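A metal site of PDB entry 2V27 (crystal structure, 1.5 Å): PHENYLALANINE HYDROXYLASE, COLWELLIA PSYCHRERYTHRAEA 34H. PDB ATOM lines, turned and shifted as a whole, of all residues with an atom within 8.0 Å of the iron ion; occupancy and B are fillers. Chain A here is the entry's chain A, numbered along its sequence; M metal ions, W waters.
ND1 of His 122 lies close to O of Gly 182.
The backbone NH (N) of His 122 sits at hydrogen-bond distance from the side-chain carboxylate (OD2) of Asp 119 (3.0 Å).
The backbone carbonyl oxygen (O) of Glu 167 is in hydrogen-bond range of the backbone NH (N) of Gly 182 (3.3 Å).
The backbone carbonyl oxygen (O) of Tyr 162 sits at hydrogen-bond distance from the backbone NH (N) of Glu 167 (3.2 Å).
A ring nitrogen (ND1) of His 122 sits at hydrogen-bond distance from the side-chain hydroxyl (OG) of Ser 186 (2.8 Å).
The backbone NH (N) of Gly 183 lies within hydrogen-bond range of the backbone carbonyl oxygen (O) of Glu 167 (2.8 Å).
O of Glu 167 is in hydrogen-bond range of N of Val 184, at 3.5 Å.
The iron ion is bound by NE2 of His 127 (2.1 Å), NE2 of His 122 (2.1 Å), water W1 (2.1 Å), water W2 (2.2 Å), OE1 of Glu 167 (2.3 Å) and OE2 of Glu 167 (2.4 Å).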
ATOM      1  N   PHE A  91       4.359 -22.386 -24.826  1.00  0.00           N
ATOM      2  CA  PHE A  91       3.485 -23.523 -24.431  1.00  0.00           C
ATOM      3  C   PHE A  91       4.229 -24.741 -23.844  1.00  0.00           C
ATOM      4  O   PHE A  91       3.954 -25.173 -22.713  1.00  0.00           O
ATOM      5  CB  PHE A  91       2.601 -23.873 -25.619  1.00  0.00           C
ATOM      6  CG  PHE A  91       1.596 -24.953 -25.301  1.00  0.00           C
ATOM      7  CD1 PHE A  91       0.428 -24.613 -24.602  1.00  0.00           C
ATOM      8  CD2 PHE A  91       1.794 -26.255 -25.723  1.00  0.00           C
ATOM      9  CE1 PHE A  91      -0.544 -25.605 -24.272  1.00  0.00           C
ATOM     10  CE2 PHE A  91       0.796 -27.288 -25.424  1.00  0.00           C
ATOM     11  CZ  PHE A  91      -0.350 -26.937 -24.693  1.00  0.00           C
ATOM     12  N   PHE A 100      -0.051 -24.572 -16.343  1.00  0.00           N
ATOM     13  CA  PHE A 100      -1.005 -24.754 -17.418  1.00  0.00           C
ATOM     14  C   PHE A 100      -1.514 -23.421 -17.967  1.00  0.00           C
ATOM     15  O   PHE A 100      -2.186 -22.703 -17.255  1.00  0.00           O
ATOM     16  CB  PHE A 100      -2.199 -25.668 -17.027  1.00  0.00           C
ATOM     17  CG  PHE A 100      -2.970 -26.144 -18.239  1.00  0.00           C
ATOM     18  CD1 PHE A 100      -2.446 -27.115 -19.045  1.00  0.00           C
ATOM     19  CD2 PHE A 100      -4.218 -25.602 -18.554  1.00  0.00           C
ATOM     20  CE1 PHE A 100      -3.131 -27.555 -20.189  1.00  0.00           C
ATOM     21  CE2 PHE A 100      -4.932 -26.058 -19.681  1.00  0.00           C
ATOM     22  CZ  PHE A 100      -4.367 -26.996 -20.493  1.00  0.00           C
ATOM     23  N   GLN A 116     -12.840 -21.591 -32.194  1.00  0.00           N
ATOM     24  CA  GLN A 116     -11.577 -22.251 -32.438  1.00  0.00           C
ATOM     25  C   GLN A 116     -10.577 -22.028 -31.295  1.00  0.00           C
ATOM     26  O   GLN A 116      -9.824 -22.932 -30.938  1.00  0.00           O
ATOM     27  CB  GLN A 116     -10.991 -21.749 -33.755  1.00  0.00           C
ATOM     28  CG  GLN A 116     -10.318 -22.888 -34.542  1.00  0.00           C
ATOM     29  OE1 GLN A 116      -8.360 -21.100 -35.647  1.00  0.00           O
ATOM     30  N   GLU A 117     -10.624 -20.830 -30.711  1.00  0.00           N
ATOM     31  CA  GLU A 117      -9.733 -20.399 -29.621  1.00  0.00           C
ATOM     32  C   GLU A 117     -10.111 -21.074 -28.313  1.00  0.00           C
ATOM     33  O   GLU A 117     -11.287 -21.187 -27.991  1.00  0.00           O
ATOM     34  CB  GLU A 117      -9.887 -18.875 -29.376  1.00  0.00           C
ATOM     35  CG  GLU A 117      -9.569 -17.977 -30.581  1.00  0.00           C
ATOM     36  CD  GLU A 117     -10.779 -17.641 -31.423  1.00  0.00           C
ATOM     37  OE1 GLU A 117     -11.756 -18.430 -31.412  1.00  0.00           O
ATOM     38  OE2 GLU A 117     -10.742 -16.595 -32.120  1.00  0.00           O
ATOM     39  N   PRO A 118      -9.127 -21.527 -27.552  1.00  0.00           N
ATOM     40  CA  PRO A 118      -9.469 -22.082 -26.246  1.00  0.00           C
ATOM     41  C   PRO A 118      -9.806 -20.953 -25.251  1.00  0.00           C
ATOM     42  O   PRO A 118      -8.910 -20.179 -24.898  1.00  0.00           O
ATOM     43  CB  PRO A 118      -8.162 -22.856 -25.855  1.00  0.00           C
ATOM     44  CG  PRO A 118      -7.084 -22.034 -26.478  1.00  0.00           C
ATOM     45  CD  PRO A 118      -7.679 -21.635 -27.834  1.00  0.00           C
ATOM     46  N   ASP A 119     -11.067 -20.844 -24.827  1.00  0.00           N
ATOM     47  CA  ASP A 119     -11.432 -19.852 -23.803  1.00  0.00           C
ATOM     48  C   ASP A 119     -11.364 -20.442 -22.386  1.00  0.00           C
ATOM     49  O   ASP A 119     -10.972 -21.618 -22.183  1.00  0.00           O
ATOM     50  CB  ASP A 119     -12.812 -19.194 -24.076  1.00  0.00           C
ATOM     51  CG  ASP A 119     -14.011 -20.116 -23.759  1.00  0.00           C
ATOM     52  OD1 ASP A 119     -15.145 -19.539 -23.738  1.00  0.00           O
ATOM     53  OD2 ASP A 119     -13.818 -21.333 -23.548  1.00  0.00           O
ATOM     54  N   HIS A 122     -13.343 -23.721 -21.805  1.00  0.00           N
ATOM     55  CA  HIS A 122     -12.583 -24.843 -22.376  1.00  0.00           C
ATOM     56  C   HIS A 122     -11.400 -25.272 -21.489  1.00  0.00           C
ATOM     57  O   HIS A 122     -11.239 -26.472 -21.167  1.00  0.00           O
ATOM     58  CB  HIS A 122     -12.077 -24.549 -23.783  1.00  0.00           C
ATOM     59  CG  HIS A 122     -11.170 -25.611 -24.302  1.00  0.00           C
ATOM     60  ND1 HIS A 122     -11.601 -26.918 -24.524  1.00  0.00           N
ATOM     61  CD2 HIS A 122      -9.834 -25.621 -24.508  1.00  0.00           C
ATOM     62  CE1 HIS A 122     -10.571 -27.647 -24.940  1.00  0.00           C
ATOM     63  NE2 HIS A 122      -9.491 -26.878 -24.945  1.00  0.00           N
ATOM     64  N   GLU A 123     -10.571 -24.314 -21.042  1.00  0.00           N
ATOM     65  CA  GLU A 123      -9.397 -24.699 -20.283  1.00  0.00           C
ATOM     66  C   GLU A 123      -9.746 -25.247 -18.897  1.00  0.00           C
ATOM     67  O   GLU A 123      -9.239 -26.309 -18.486  1.00  0.00           O
ATOM     68  CB  GLU A 123      -8.458 -23.459 -20.142  1.00  0.00           C
ATOM     69  CG  GLU A 123      -7.992 -22.836 -21.437  1.00  0.00           C
ATOM     70  CD  GLU A 123      -7.081 -23.744 -22.270  1.00  0.00           C
ATOM     71  OE1 GLU A 123      -7.055 -25.006 -22.131  1.00  0.00           O
ATOM     72  OE2 GLU A 123      -6.364 -23.207 -23.129  1.00  0.00           O
ATOM     73  N   GLY A 126     -12.635 -28.092 -19.340  1.00  0.00           N
ATOM     74  CA  GLY A 126     -12.214 -29.204 -20.171  1.00  0.00           C
ATOM     75  C   GLY A 126     -10.929 -29.877 -19.730  1.00  0.00           C
ATOM     76  O   GLY A 126     -10.838 -31.121 -19.752  1.00  0.00           O
ATOM     77  N   HIS A 127      -9.908 -29.092 -19.350  1.00  0.00           N
ATOM     78  CA  HIS A 127      -8.614 -29.711 -19.108  1.00  0.00           C
ATOM     79  C   HIS A 127      -8.237 -29.754 -17.618  1.00  0.00           C
ATOM     80  O   HIS A 127      -7.629 -30.733 -17.129  1.00  0.00           O
ATOM     81  CB  HIS A 127      -7.494 -28.957 -19.824  1.00  0.00           C
ATOM     82  CG  HIS A 127      -7.533 -29.077 -21.317  1.00  0.00           C
ATOM     83  ND1 HIS A 127      -7.406 -30.281 -21.966  1.00  0.00           N
ATOM     84  CD2 HIS A 127      -7.658 -28.136 -22.279  1.00  0.00           C
ATOM     85  CE1 HIS A 127      -7.435 -30.072 -23.281  1.00  0.00           C
ATOM     86  NE2 HIS A 127      -7.581 -28.779 -23.504  1.00  0.00           N
ATOM     87  N   TYR A 162      -0.215 -34.789 -28.723  1.00  0.00           N
ATOM     88  CA  TYR A 162      -1.096 -33.945 -27.867  1.00  0.00           C
ATOM     89  C   TYR A 162      -2.583 -34.009 -28.323  1.00  0.00           C
ATOM     90  O   TYR A 162      -3.480 -34.243 -27.507  1.00  0.00           O
ATOM     91  CB  TYR A 162      -0.620 -32.516 -27.907  1.00  0.00           C
ATOM     92  CG  TYR A 162      -1.264 -31.652 -26.838  1.00  0.00           C
ATOM     93  CD1 TYR A 162      -0.687 -31.604 -25.570  1.00  0.00           C
ATOM     94  CD2 TYR A 162      -2.404 -30.858 -27.120  1.00  0.00           C
ATOM     95  CE1 TYR A 162      -1.166 -30.742 -24.569  1.00  0.00           C
ATOM     96  CE2 TYR A 162      -2.925 -30.004 -26.064  1.00  0.00           C
ATOM     97  CZ  TYR A 162      -2.263 -30.012 -24.819  1.00  0.00           C
ATOM     98  OH  TYR A 162      -2.620 -29.246 -23.677  1.00  0.00           O
ATOM     99  N   TRP A 163      -2.800 -33.806 -29.617  1.00  0.00           N
ATOM    100  CA  TRP A 163      -4.115 -33.764 -30.205  1.00  0.00           C
ATOM    101  C   TRP A 163      -4.884 -35.070 -29.828  1.00  0.00           C
ATOM    102  O   TRP A 163      -6.032 -35.002 -29.432  1.00  0.00           O
ATOM    103  CB  TRP A 163      -3.997 -33.685 -31.711  1.00  0.00           C
ATOM    104  CG  TRP A 163      -5.315 -33.536 -32.444  1.00  0.00           C
ATOM    105  CD1 TRP A 163      -6.004 -34.499 -33.149  1.00  0.00           C
ATOM    106  CD2 TRP A 163      -6.097 -32.329 -32.506  1.00  0.00           C
ATOM    107  NE1 TRP A 163      -7.155 -33.929 -33.687  1.00  0.00           N
ATOM    108  CE2 TRP A 163      -7.242 -32.618 -33.283  1.00  0.00           C
ATOM    109  CE3 TRP A 163      -5.934 -31.007 -31.991  1.00  0.00           C
ATOM    110  CZ2 TRP A 163      -8.241 -31.638 -33.579  1.00  0.00           C
ATOM    111  CZ3 TRP A 163      -6.900 -30.037 -32.289  1.00  0.00           C
ATOM    112  CH2 TRP A 163      -8.051 -30.362 -33.088  1.00  0.00           C
ATOM    113  N   ILE A 166      -4.396 -35.445 -24.979  1.00  0.00           N
ATOM    114  CA  ILE A 166      -4.926 -34.378 -24.125  1.00  0.00           C
ATOM    115  C   ILE A 166      -6.185 -33.718 -24.719  1.00  0.00           C
ATOM    116  O   ILE A 166      -7.088 -33.307 -23.969  1.00  0.00           O
ATOM    117  CB  ILE A 166      -3.788 -33.316 -23.857  1.00  0.00           C
ATOM    118  CG1 ILE A 166      -2.796 -34.023 -22.925  1.00  0.00           C
ATOM    119  CG2 ILE A 166      -4.317 -32.003 -23.189  1.00  0.00           C
ATOM    120  CD1 ILE A 166      -1.382 -33.436 -22.837  1.00  0.00           C
ATOM    121  N   GLU A 167      -6.232 -33.547 -26.051  1.00  0.00           N
ATOM    122  CA  GLU A 167      -7.394 -32.864 -26.652  1.00  0.00           C
ATOM    123  C   GLU A 167      -8.562 -33.824 -26.964  1.00  0.00           C
ATOM    124  O   GLU A 167      -9.705 -33.512 -26.639  1.00  0.00           O
ATOM    125  CB  GLU A 167      -7.036 -32.048 -27.880  1.00  0.00           C
ATOM    126  CG  GLU A 167      -6.107 -30.928 -27.534  1.00  0.00           C
ATOM    127  CD  GLU A 167      -6.754 -29.806 -26.685  1.00  0.00           C
ATOM    128  OE1 GLU A 167      -5.979 -29.015 -26.158  1.00  0.00           O
ATOM    129  OE2 GLU A 167      -8.000 -29.667 -26.594  1.00  0.00           O
ATOM    130  N   PHE A 168      -8.251 -34.952 -27.686  1.00  0.00           N
ATOM    131  CA  PHE A 168      -9.316 -35.842 -28.226  1.00  0.00           C
ATOM    132  C   PHE A 168      -9.243 -37.250 -27.748  1.00  0.00           C
ATOM    133  O   PHE A 168      -9.873 -38.155 -28.323  1.00  0.00           O
ATOM    134  CB  PHE A 168      -9.391 -35.715 -29.777  1.00  0.00           C
ATOM    135  CG  PHE A 168      -9.999 -34.408 -30.168  1.00  0.00           C
ATOM    136  CD1 PHE A 168      -9.175 -33.287 -30.358  1.00  0.00           C
ATOM    137  CD2 PHE A 168     -11.367 -34.249 -30.256  1.00  0.00           C
ATOM    138  CE1 PHE A 168      -9.767 -32.019 -30.670  1.00  0.00           C
ATOM    139  CE2 PHE A 168     -11.979 -33.009 -30.553  1.00  0.00           C
ATOM    140  CZ  PHE A 168     -11.160 -31.884 -30.735  1.00  0.00           C
ATOM    141  N   GLY A 181     -10.311 -36.573 -23.346  1.00  0.00           N
ATOM    142  CA  GLY A 181      -9.813 -35.367 -24.040  1.00  0.00           C
ATOM    143  C   GLY A 181     -10.638 -34.108 -23.738  1.00  0.00           C
ATOM    144  O   GLY A 181     -11.862 -34.065 -23.862  1.00  0.00           O
ATOM    145  N   GLY A 182      -9.920 -33.019 -23.432  1.00  0.00           N
ATOM    146  CA  GLY A 182     -10.585 -31.758 -23.053  1.00  0.00           C
ATOM    147  C   GLY A 182     -11.349 -31.053 -24.182  1.00  0.00           C
ATOM    148  O   GLY A 182     -12.319 -30.283 -23.914  1.00  0.00           O
ATOM    149  N   GLY A 183     -10.895 -31.268 -25.423  1.00  0.00           N
ATOM    150  CA  GLY A 183     -11.581 -30.771 -26.615  1.00  0.00           C
ATOM    151  C   GLY A 183     -12.966 -31.370 -26.806  1.00  0.00           C
ATOM    152  O   GLY A 183     -13.898 -30.752 -27.358  1.00  0.00           O
ATOM    153  N   VAL A 184     -13.071 -32.606 -26.339  1.00  0.00           N
ATOM    154  CA  VAL A 184     -14.361 -33.288 -26.372  1.00  0.00           C
ATOM    155  C   VAL A 184     -15.230 -32.861 -25.184  1.00  0.00           C
ATOM    156  O   VAL A 184     -16.401 -32.459 -25.346  1.00  0.00           O
ATOM    157  CB  VAL A 184     -14.155 -34.791 -26.372  1.00  0.00           C
ATOM    158  CG1 VAL A 184     -15.463 -35.543 -26.493  1.00  0.00           C
ATOM    159  CG2 VAL A 184     -13.183 -35.221 -27.551  1.00  0.00           C
ATOM    160  N   SER A 186     -15.499 -30.344 -23.221  1.00  0.00           N
ATOM    161  CA  SER A 186     -16.002 -28.964 -23.037  1.00  0.00           C
ATOM    162  C   SER A 186     -17.064 -28.592 -24.078  1.00  0.00           C
ATOM    163  O   SER A 186     -17.602 -27.467 -24.035  1.00  0.00           O
ATOM    164  CB  SER A 186     -14.883 -27.925 -23.057  1.00  0.00           C
ATOM    165  OG  SER A 186     -14.187 -27.943 -24.286  1.00  0.00           O
HETATM  166 FE    FE M   1      -7.617 -27.741 -25.281  1.00  0.00          FE
HETATM  167  O   HOH W   1      -7.304 -26.702 -27.100  1.00  0.00           O
HETATM  168  O   HOH W   2      -6.320 -26.226 -24.437  1.00  0.00           O
